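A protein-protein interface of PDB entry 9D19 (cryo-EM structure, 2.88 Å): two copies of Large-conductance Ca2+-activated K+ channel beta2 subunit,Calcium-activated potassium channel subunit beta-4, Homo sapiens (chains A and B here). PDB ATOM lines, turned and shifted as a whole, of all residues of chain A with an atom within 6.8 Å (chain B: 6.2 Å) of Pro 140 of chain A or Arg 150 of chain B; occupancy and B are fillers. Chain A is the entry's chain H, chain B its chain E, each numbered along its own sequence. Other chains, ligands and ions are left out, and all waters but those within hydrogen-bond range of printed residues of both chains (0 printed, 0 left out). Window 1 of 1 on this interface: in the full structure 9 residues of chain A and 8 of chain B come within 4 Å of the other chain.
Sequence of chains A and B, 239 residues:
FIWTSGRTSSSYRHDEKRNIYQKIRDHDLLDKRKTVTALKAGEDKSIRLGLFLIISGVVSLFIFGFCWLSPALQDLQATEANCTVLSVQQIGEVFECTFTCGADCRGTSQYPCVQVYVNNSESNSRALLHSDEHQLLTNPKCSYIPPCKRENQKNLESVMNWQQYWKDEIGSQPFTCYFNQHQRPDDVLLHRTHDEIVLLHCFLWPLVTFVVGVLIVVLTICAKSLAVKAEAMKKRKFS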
ATOM      1  N   GLN A 115      -6.920  -4.680   8.413  1.00  0.00           N
ATOM      2  CA  GLN A 115      -7.115  -3.371   9.015  1.00  0.00           C
ATOM      3  C   GLN A 115      -8.012  -3.509  10.241  1.00  0.00           C
ATOM      4  O   GLN A 115      -8.923  -4.335  10.279  1.00  0.00           O
ATOM      5  CB  GLN A 115      -7.671  -2.372   8.001  1.00  0.00           C
ATOM      6  CG  GLN A 115      -6.628  -1.993   6.939  1.00  0.00           C
ATOM      7  CD  GLN A 115      -7.082  -0.823   6.068  1.00  0.00           C
ATOM      8  OE1 GLN A 115      -8.235  -0.413   6.072  1.00  0.00           O
ATOM      9  NE2 GLN A 115      -6.204  -0.222   5.296  1.00  0.00           N
ATOM     10  N   TYR A 117     -10.012  -0.924  13.205  1.00  0.00           N
ATOM     11  CA  TYR A 117     -10.417   0.444  13.515  1.00  0.00           C
ATOM     12  C   TYR A 117     -10.926   0.530  14.945  1.00  0.00           C
ATOM     13  O   TYR A 117     -11.501  -0.426  15.470  1.00  0.00           O
ATOM     14  CB  TYR A 117     -11.428   0.940  12.484  1.00  0.00           C
ATOM     15  CG  TYR A 117     -10.826   1.135  11.106  1.00  0.00           C
ATOM     16  CD1 TYR A 117     -10.246   2.372  10.770  1.00  0.00           C
ATOM     17  CD2 TYR A 117     -10.830   0.090  10.165  1.00  0.00           C
ATOM     18  CE1 TYR A 117      -9.715   2.583   9.488  1.00  0.00           C
ATOM     19  CE2 TYR A 117     -10.285   0.292   8.882  1.00  0.00           C
ATOM     20  CZ  TYR A 117      -9.733   1.543   8.541  1.00  0.00           C
ATOM     21  OH  TYR A 117      -9.215   1.759   7.305  1.00  0.00           O
ATOM     22  N   LEU A 128      -7.264   4.194  12.705  1.00  0.00           N
ATOM     23  CA  LEU A 128      -6.719   2.884  12.329  1.00  0.00           C
ATOM     24  C   LEU A 128      -5.656   2.448  13.338  1.00  0.00           C
ATOM     25  O   LEU A 128      -4.719   3.184  13.641  1.00  0.00           O
ATOM     26  CB  LEU A 128      -6.161   2.989  10.900  1.00  0.00           C
ATOM     27  CG  LEU A 128      -5.340   1.792  10.379  1.00  0.00           C
ATOM     28  CD1 LEU A 128      -6.068   0.454  10.437  1.00  0.00           C
ATOM     29  CD2 LEU A 128      -4.996   2.037   8.912  1.00  0.00           C
ATOM     30  N   HIS A 130      -2.423   0.414  14.692  1.00  0.00           N
ATOM     31  CA  HIS A 130      -1.109   0.024  14.260  1.00  0.00           C
ATOM     32  C   HIS A 130      -0.347  -0.493  15.467  1.00  0.00           C
ATOM     33  O   HIS A 130      -0.210   0.197  16.391  1.00  0.00           O
ATOM     34  CB  HIS A 130      -0.418   1.217  13.664  1.00  0.00           C
ATOM     35  CG  HIS A 130      -0.858   1.604  12.304  1.00  0.00           C
ATOM     36  ND1 HIS A 130      -0.520   0.968  11.156  1.00  0.00           N
ATOM     37  CD2 HIS A 130      -1.699   2.607  11.965  1.00  0.00           C
ATOM     38  CE1 HIS A 130      -1.099   1.594  10.141  1.00  0.00           C
ATOM     39  NE2 HIS A 130      -1.827   2.614  10.581  1.00  0.00           N
ATOM     40  N   GLN A 135       5.668  -0.603  13.012  1.00  0.00           N
ATOM     41  CA  GLN A 135       4.645  -1.163  12.136  1.00  0.00           C
ATOM     42  C   GLN A 135       3.946  -0.059  11.331  1.00  0.00           C
ATOM     43  O   GLN A 135       3.844  -0.172  10.109  1.00  0.00           O
ATOM     44  CB  GLN A 135       3.668  -2.031  12.939  1.00  0.00           C
ATOM     45  CG  GLN A 135       2.789  -2.906  12.034  1.00  0.00           C
ATOM     46  CD  GLN A 135       1.702  -2.145  11.285  1.00  0.00           C
ATOM     47  OE1 GLN A 135       1.072  -1.240  11.799  1.00  0.00           O
ATOM     48  NE2 GLN A 135       1.441  -2.472  10.039  1.00  0.00           N
ATOM     49  N   LEU A 136       3.548   1.039  11.982  1.00  0.00           N
ATOM     50  CA  LEU A 136       2.980   2.208  11.307  1.00  0.00           C
ATOM     51  C   LEU A 136       3.898   2.696  10.184  1.00  0.00           C
ATOM     52  O   LEU A 136       3.431   2.969   9.092  1.00  0.00           O
ATOM     53  CB  LEU A 136       2.713   3.324  12.333  1.00  0.00           C
ATOM     54  CG  LEU A 136       2.393   4.707  11.742  1.00  0.00           C
ATOM     55  CD1 LEU A 136       1.128   4.722  10.899  1.00  0.00           C
ATOM     56  CD2 LEU A 136       2.204   5.719  12.868  1.00  0.00           C
ATOM     57  N   LEU A 137       5.204   2.803  10.424  1.00  0.00           N
ATOM     58  CA  LEU A 137       6.127   3.341   9.433  1.00  0.00           C
ATOM     59  C   LEU A 137       6.568   2.316   8.377  1.00  0.00           C
ATOM     60  O   LEU A 137       6.816   2.702   7.237  1.00  0.00           O
ATOM     61  CB  LEU A 137       7.299   3.994  10.174  1.00  0.00           C
ATOM     62  CG  LEU A 137       6.910   5.272  10.945  1.00  0.00           C
ATOM     63  CD1 LEU A 137       8.095   5.753  11.776  1.00  0.00           C
ATOM     64  CD2 LEU A 137       6.505   6.407  10.004  1.00  0.00           C
ATOM     65  N   THR A 138       6.654   1.018   8.688  1.00  0.00           N
ATOM     66  CA  THR A 138       7.014  -0.012   7.695  1.00  0.00           C
ATOM     67  C   THR A 138       5.872  -0.322   6.720  1.00  0.00           C
ATOM     68  O   THR A 138       6.128  -0.626   5.557  1.00  0.00           O
ATOM     69  CB  THR A 138       7.566  -1.289   8.358  1.00  0.00           C
ATOM     70  OG1 THR A 138       8.313  -2.025   7.418  1.00  0.00           O
ATOM     71  CG2 THR A 138       6.504  -2.250   8.882  1.00  0.00           C
ATOM     72  N   ASN A 139       4.608  -0.194   7.151  1.00  0.00           N
ATOM     73  CA  ASN A 139       3.438  -0.317   6.280  1.00  0.00           C
ATOM     74  C   ASN A 139       2.228   0.481   6.825  1.00  0.00           C
ATOM     75  O   ASN A 139       1.313  -0.098   7.410  1.00  0.00           O
ATOM     76  CB  ASN A 139       3.110  -1.805   6.060  1.00  0.00           C
ATOM     77  CG  ASN A 139       2.066  -1.997   4.973  1.00  0.00           C
ATOM     78  OD1 ASN A 139       1.467  -1.060   4.473  1.00  0.00           O
ATOM     79  ND2 ASN A 139       1.836  -3.212   4.550  1.00  0.00           N
ATOM     80  N   PRO A 140       2.163   1.805   6.602  1.00  0.00           N
ATOM     81  CA  PRO A 140       1.084   2.654   7.120  1.00  0.00           C
ATOM     82  C   PRO A 140      -0.286   2.356   6.511  1.00  0.00           C
ATOM     83  O   PRO A 140      -1.316   2.722   7.073  1.00  0.00           O
ATOM     84  CB  PRO A 140       1.509   4.089   6.810  1.00  0.00           C
ATOM     85  CG  PRO A 140       2.493   3.938   5.653  1.00  0.00           C
ATOM     86  CD  PRO A 140       3.161   2.597   5.909  1.00  0.00           C
ATOM     87  N   LYS A 141      -0.315   1.669   5.371  1.00  0.00           N
ATOM     88  CA  LYS A 141      -1.514   1.173   4.686  1.00  0.00           C
ATOM     89  C   LYS A 141      -2.157  -0.032   5.404  1.00  0.00           C
ATOM     90  O   LYS A 141      -3.293  -0.381   5.085  1.00  0.00           O
ATOM     91  CB  LYS A 141      -1.056   0.918   3.233  1.00  0.00           C
ATOM     92  CG  LYS A 141      -1.857  -0.005   2.321  1.00  0.00           C
ATOM     93  CD  LYS A 141      -3.149   0.569   1.724  1.00  0.00           C
ATOM     94  CE  LYS A 141      -3.561  -0.463   0.665  1.00  0.00           C
ATOM     95  NZ  LYS A 141      -4.705  -0.078  -0.191  1.00  0.00           N
ATOM     96  N   CYS A 142      -1.495  -0.647   6.392  1.00  0.00           N
ATOM     97  CA  CYS A 142      -1.929  -1.904   7.012  1.00  0.00           C
ATOM     98  C   CYS A 142      -1.762  -1.942   8.547  1.00  0.00           C
ATOM     99  O   CYS A 142      -0.920  -1.236   9.089  1.00  0.00           O
ATOM    100  CB  CYS A 142      -1.152  -3.035   6.333  1.00  0.00           C
ATOM    101  SG  CYS A 142      -1.965  -4.620   6.534  1.00  0.00           S
ATOM    102  N   SER A 143      -2.541  -2.753   9.275  1.00  0.00           N
ATOM    103  CA  SER A 143      -2.624  -2.697  10.754  1.00  0.00           C
ATOM    104  C   SER A 143      -1.655  -3.607  11.527  1.00  0.00           C
ATOM    105  O   SER A 143      -1.309  -3.327  12.674  1.00  0.00           O
ATOM    106  CB  SER A 143      -4.063  -3.020  11.152  1.00  0.00           C
ATOM    107  OG  SER A 143      -4.267  -2.962  12.537  1.00  0.00           O
ATOM    108  N   ASP A 186      -5.120  10.139  12.526  1.00  0.00           N
ATOM    109  CA  ASP A 186      -6.121   9.070  12.503  1.00  0.00           C
ATOM    110  C   ASP A 186      -5.469   7.675  12.617  1.00  0.00           C
ATOM    111  O   ASP A 186      -5.993   6.684  12.107  1.00  0.00           O
ATOM    112  CB  ASP A 186      -7.083   9.231  11.307  1.00  0.00           C
ATOM    113  CG  ASP A 186      -6.446   9.346   9.909  1.00  0.00           C
ATOM    114  OD1 ASP A 186      -5.218   9.190   9.749  1.00  0.00           O
ATOM    115  OD2 ASP A 186      -7.209   9.617   8.949  1.00  0.00           O
ATOM    116  N   ASP A 187      -4.343   7.593  13.339  1.00  0.00           N
ATOM    117  CA  ASP A 187      -3.568   6.369  13.591  1.00  0.00           C
ATOM    118  C   ASP A 187      -3.348   6.148  15.100  1.00  0.00           C
ATOM    119  O   ASP A 187      -3.074   7.093  15.833  1.00  0.00           O
ATOM    120  CB  ASP A 187      -2.217   6.390  12.854  1.00  0.00           C
ATOM    121  CG  ASP A 187      -2.294   6.239  11.330  1.00  0.00           C
ATOM    122  OD1 ASP A 187      -3.359   5.832  10.820  1.00  0.00           O
ATOM    123  OD2 ASP A 187      -1.305   6.580  10.648  1.00  0.00           O
ATOM    124  N   PHE B  99       1.084   8.717  -0.185  1.00  0.00           N
ATOM    125  CA  PHE B  99       0.426   9.316   0.979  1.00  0.00           C
ATOM    126  C   PHE B  99       1.375   9.346   2.177  1.00  0.00           C
ATOM    127  O   PHE B  99       2.224   8.471   2.336  1.00  0.00           O
ATOM    128  CB  PHE B  99      -0.886   8.596   1.312  1.00  0.00           C
ATOM    129  CG  PHE B  99      -0.742   7.206   1.891  1.00  0.00           C
ATOM    130  CD1 PHE B  99      -0.578   6.106   1.032  1.00  0.00           C
ATOM    131  CD2 PHE B  99      -0.811   7.000   3.281  1.00  0.00           C
ATOM    132  CE1 PHE B  99      -0.487   4.810   1.561  1.00  0.00           C
ATOM    133  CE2 PHE B  99      -0.737   5.702   3.808  1.00  0.00           C
ATOM    134  CZ  PHE B  99      -0.581   4.605   2.947  1.00  0.00           C
ATOM    135  N   THR B 100       1.254  10.379   3.003  1.00  0.00           N
ATOM    136  CA  THR B 100       2.262  10.771   3.998  1.00  0.00           C
ATOM    137  C   THR B 100       1.696  10.761   5.417  1.00  0.00           C
ATOM    138  O   THR B 100       0.505  10.958   5.632  1.00  0.00           O
ATOM    139  CB  THR B 100       2.865  12.137   3.652  1.00  0.00           C
ATOM    140  OG1 THR B 100       1.879  13.128   3.588  1.00  0.00           O
ATOM    141  CG2 THR B 100       3.573  12.126   2.311  1.00  0.00           C
ATOM    142  N   CYS B 101       2.588  10.510   6.390  1.00  0.00           N
ATOM    143  CA  CYS B 101       2.215  10.409   7.814  1.00  0.00           C
ATOM    144  C   CYS B 101       3.244  10.783   8.914  1.00  0.00           C
ATOM    145  O   CYS B 101       3.442   9.996   9.840  1.00  0.00           O
ATOM    146  CB  CYS B 101       1.716   8.983   8.120  1.00  0.00           C
ATOM    147  SG  CYS B 101       2.842   7.622   7.689  1.00  0.00           S
ATOM    148  N   CYS B 105       7.404   8.539   6.719  1.00  0.00           N
ATOM    149  CA  CYS B 105       6.449   7.445   6.955  1.00  0.00           C
ATOM    150  C   CYS B 105       5.815   6.828   5.692  1.00  0.00           C
ATOM    151  O   CYS B 105       5.091   5.840   5.774  1.00  0.00           O
ATOM    152  CB  CYS B 105       5.417   8.000   7.945  1.00  0.00           C
ATOM    153  SG  CYS B 105       4.026   6.964   8.438  1.00  0.00           S
ATOM    154  N   ARG B 106       6.015   7.443   4.523  1.00  0.00           N
ATOM    155  CA  ARG B 106       5.131   7.313   3.353  1.00  0.00           C
ATOM    156  C   ARG B 106       4.884   5.892   2.822  1.00  0.00           C
ATOM    157  O   ARG B 106       5.759   5.026   2.884  1.00  0.00           O
ATOM    158  CB  ARG B 106       5.597   8.278   2.245  1.00  0.00           C
ATOM    159  CG  ARG B 106       6.966   8.025   1.586  1.00  0.00           C
ATOM    160  CD  ARG B 106       7.413   9.073   0.561  1.00  0.00           C
ATOM    161  NE  ARG B 106       8.707   8.734  -0.057  1.00  0.00           N
ATOM    162  CZ  ARG B 106       9.909   8.968   0.427  1.00  0.00           C
ATOM    163  NH1 ARG B 106      10.962   8.738  -0.303  1.00  0.00           N
ATOM    164  NH2 ARG B 106      10.100   9.415   1.629  1.00  0.00           N
ATOM    165  N   GLY B 107       3.718   5.698   2.213  1.00  0.00           N
ATOM    166  CA  GLY B 107       3.355   4.528   1.400  1.00  0.00           C
ATOM    167  C   GLY B 107       2.623   4.939   0.120  1.00  0.00           C
ATOM    168  O   GLY B 107       2.430   6.132  -0.112  1.00  0.00           O
ATOM    169  N   THR B 108       2.193   3.989  -0.715  1.00  0.00           N
ATOM    170  CA  THR B 108       1.480   4.306  -1.969  1.00  0.00           C
ATOM    171  C   THR B 108       0.081   3.703  -2.055  1.00  0.00           C
ATOM    172  O   THR B 108      -0.211   2.630  -1.518  1.00  0.00           O
ATOM    173  CB  THR B 108       2.287   3.986  -3.236  1.00  0.00           C
ATOM    174  OG1 THR B 108       2.454   2.604  -3.422  1.00  0.00           O
ATOM    175  CG2 THR B 108       3.670   4.629  -3.238  1.00  0.00           C
ATOM    176  N   SER B 109      -0.796   4.421  -2.749  1.00  0.00           N
ATOM    177  CA  SER B 109      -2.194   4.067  -2.990  1.00  0.00           C
ATOM    178  C   SER B 109      -2.548   4.317  -4.446  1.00  0.00           C
ATOM    179  O   SER B 109      -2.047   5.257  -5.059  1.00  0.00           O
ATOM    180  CB  SER B 109      -3.118   4.878  -2.087  1.00  0.00           C
ATOM    181  OG  SER B 109      -2.882   4.564  -0.736  1.00  0.00           O
ATOM    182  N   CYS B 148      -3.459  12.407  -2.338  1.00  0.00           N
ATOM    183  CA  CYS B 148      -3.488  11.095  -1.718  1.00  0.00           C
ATOM    184  C   CYS B 148      -3.928  11.140  -0.262  1.00  0.00           C
ATOM    185  O   CYS B 148      -3.213  11.649   0.601  1.00  0.00           O
ATOM    186  CB  CYS B 148      -2.106  10.453  -1.844  1.00  0.00           C
ATOM    187  SG  CYS B 148      -1.572  10.085  -3.530  1.00  0.00           S
ATOM    188  N   LYS B 149      -5.108  10.568  -0.029  1.00  0.00           N
ATOM    189  CA  LYS B 149      -5.723  10.503   1.286  1.00  0.00           C
ATOM    190  C   LYS B 149      -5.959   9.068   1.758  1.00  0.00           C
ATOM    191  O   LYS B 149      -7.094   8.588   1.779  1.00  0.00           O
ATOM    192  CB  LYS B 149      -7.044  11.274   1.291  1.00  0.00           C
ATOM    193  CG  LYS B 149      -6.890  12.768   1.066  1.00  0.00           C
ATOM    194  CD  LYS B 149      -8.239  13.468   1.084  1.00  0.00           C
ATOM    195  CE  LYS B 149      -8.093  14.955   0.809  1.00  0.00           C
ATOM    196  NZ  LYS B 149      -7.293  15.637   1.865  1.00  0.00           N
ATOM    197  N   ARG B 150      -4.855   8.405   2.101  1.00  0.00           N
ATOM    198  CA  ARG B 150      -4.812   7.023   2.596  1.00  0.00           C
ATOM    199  C   ARG B 150      -5.294   5.915   1.649  1.00  0.00           C
ATOM    200  O   ARG B 150      -4.546   5.467   0.780  1.00  0.00           O
ATOM    201  CB  ARG B 150      -5.479   6.893   3.976  1.00  0.00           C
ATOM    202  CG  ARG B 150      -4.805   7.706   5.070  1.00  0.00           C
ATOM    203  CD  ARG B 150      -3.389   7.221   5.331  1.00  0.00           C
ATOM    204  NE  ARG B 150      -3.365   5.831   5.775  1.00  0.00           N
ATOM    205  CZ  ARG B 150      -3.584   5.445   7.028  1.00  0.00           C
ATOM    206  NH1 ARG B 150      -3.544   4.157   7.342  1.00  0.00           N
ATOM    207  NH2 ARG B 150      -3.841   6.344   7.967  1.00  0.00           N
ATOM    208  N   GLU B 151      -6.536   5.478   1.824  1.00  0.00           N
ATOM    209  CA  GLU B 151      -7.090   4.372   1.038  1.00  0.00           C
ATOM    210  C   GLU B 151      -7.605   4.659  -0.376  1.00  0.00           C
ATOM    211  O   GLU B 151      -8.149   5.723  -0.665  1.00  0.00           O
ATOM    212  CB  GLU B 151      -8.182   3.658   1.841  1.00  0.00           C
ATOM    213  CG  GLU B 151      -9.337   4.554   2.252  1.00  0.00           C
ATOM    214  CD  GLU B 151      -9.173   5.110   3.653  1.00  0.00           C
ATOM    215  OE1 GLU B 151      -8.484   4.465   4.473  1.00  0.00           O
ATOM    216  OE2 GLU B 151      -9.732   6.190   3.935  1.00  0.00           O
ATOM    217  N   ASN B 152      -7.420   3.661  -1.236  1.00  0.00           N
ATOM    218  CA  ASN B 152      -7.857   3.666  -2.637  1.00  0.00           C
ATOM    219  C   ASN B 152      -9.300   4.149  -2.841  1.00  0.00           C
ATOM    220  O   ASN B 152      -9.583   4.866  -3.800  1.00  0.00           O
ATOM    221  CB  ASN B 152      -7.712   2.249  -3.208  1.00  0.00           C
ATOM    222  CG  ASN B 152      -6.285   1.773  -3.388  1.00  0.00           C
ATOM    223  OD1 ASN B 152      -5.316   2.428  -3.035  1.00  0.00           O
ATOM    224  ND2 ASN B 152      -6.110   0.612  -3.963  1.00  0.00           N
ATOM    225  N   LYS B 154     -11.042   6.432  -1.230  1.00  0.00           N
ATOM    226  CA  LYS B 154     -11.118   7.896  -1.143  1.00  0.00           C
ATOM    227  C   LYS B 154     -10.491   8.575  -2.360  1.00  0.00           C
ATOM    228  O   LYS B 154     -10.991   9.598  -2.816  1.00  0.00           O
ATOM    229  CB  LYS B 154     -10.448   8.375   0.151  1.00  0.00           C
ATOM    230  CG  LYS B 154     -11.041   7.800   1.442  1.00  0.00           C
ATOM    231  CD  LYS B 154     -12.523   8.131   1.630  1.00  0.00           C
ATOM    232  CE  LYS B 154     -12.998   7.842   3.055  1.00  0.00           C
ATOM    233  NZ  LYS B 154     -12.932   6.409   3.415  1.00  0.00           N
ATOM    234  N   ASN B 155      -9.444   7.985  -2.937  1.00  0.00           N
ATOM    235  CA  ASN B 155      -8.885   8.454  -4.206  1.00  0.00           C
ATOM    236  C   ASN B 155      -9.893   8.286  -5.349  1.00  0.00           C
ATOM    237  O   ASN B 155     -10.149   9.237  -6.082  1.00  0.00           O
ATOM    238  CB  ASN B 155      -7.584   7.709  -4.522  1.00  0.00           C
ATOM    239  CG  ASN B 155      -6.431   8.024  -3.602  1.00  0.00           C
ATOM    240  OD1 ASN B 155      -6.435   8.978  -2.846  1.00  0.00           O
ATOM    241  ND2 ASN B 155      -5.393   7.233  -3.668  1.00  0.00           N
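Among the printed residues, merely in contact across the chains: Leu 137 of chain A with Cys 105 of chain B (2.8 Å), Leu 128 of chain A with Arg 150 of chain B (3.0 Å), Pro 140 of chain A with Cys 105 of chain B (3.2 Å), Lys 141 of chain A with Phe 99 of chain B (3.7 Å), Lys 141 of chain A with Asn 152 of chain B (3.8 Å), Pro 140 of chain A with Cys 101 of chain B (3.9 Å), His 130 of chain A with Arg 150 of chain B (3.98 Å) and Tyr 117 of chain A with Glu 151 of chain B (3.98 Å).
No position is printed for both chains. Of the 11 pairs that touch across the chains among the printed residues, none has its exchanged pair printed and touching as well.
The side-chain carboxylate of Asp 187 of chain A is in salt-bridge range of the guanidinium group of Arg 150 of chain B, at 2.9 Å. The guanidinium group of Arg 150 of chain B lies within salt-bridge range of the side-chain carboxylate of Asp 186 of chain A. O of Pro 140 of chain A sits at hydrogen-bond distance from NH1 of Arg 150 of chain B, at 2.7 Å.
Of the 15 printed residues of chain B, 6 touch a printed residue of chain A. Hydrophobic or aromatic side chains of chain B that line the printed part of chain A: Phe 99. Of the 15 printed residues of chain A, 8 touch a printed residue of chain B. Printed residues of chain A that touch a printed residue of chain B: Tyr 117, Leu 128, His 130, Leu 137, Pro 140, Lys 141, Asp 186 and Asp 187. Hydrophobic or aromatic side chains of chain A within 4 Å of the printed part of chain B: Tyr 117, Leu 128, His 130, Leu 137 and Pro 140. Among the printed residues, Asp or Glu carboxylates within 4 Å of a Lys or Arg side-chain nitrogen of the other chain: Asp 186 of chain A with Arg 150 of chain B and Asp 187 of chain A with Arg 150 of chain B.
ND1 of His 130 of chain A is in hydrogen-bond range of OE1 of Gln 135 of chain A (2.8 Å). A ring nitrogen (ND1) of His 130 of chain A lies close to the backbone carbonyl oxygen of Cys 142 of chain A, 3.0 Å away. N of Leu 128 of chain A is in hydrogen-bond range of O of Asp 186 of chain A. O of Arg 150 of chain B lies within hydrogen-bond range of OG of Ser 109 of chain B, at 2.4 Å. NE2 of Gln 115 of chain A lies within hydrogen-bond range of O of Lys 141 of chain A, at 2.9 Å. NZ of Lys 154 of chain B lies within salt-bridge range of OE2 of Glu 151 of chain B (3.2 Å).
Pro 140 of chain A touches just these residues of chain B: Cys 101 (3.9 Å), Cys 105 (3.2 Å) and Arg 150 (2.7 Å). Arg 150 of chain B touches just these residues of chain A: Leu 128, His 130, Pro 140, Asp 186 and Asp 187. Of the printed residues of chain A, Phe 99 of chain B touches Lys 141. Of the printed residues of chain B, Asp 187 of chain A touches Arg 150 (2.9 Å). Printed residues of chain B within 4 Å of Tyr 117 of chain A: Glu 151. Of the printed residues of chain B, Leu 137 of chain A touches Cys 105 (2.8 Å). Printed residues of chain B within 4 Å of His 130 of chain A: Arg 150. Leu 136 of chain A touches none of the printed residues of chain B. The nearest printed residue of chain B that does not touch Pro 140 of chain A is Gly 107 of chain B (4.1 Å). The nearest printed residue of chain B that does not touch His 130 of chain A is Cys 101 of chain B (7.4 Å).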
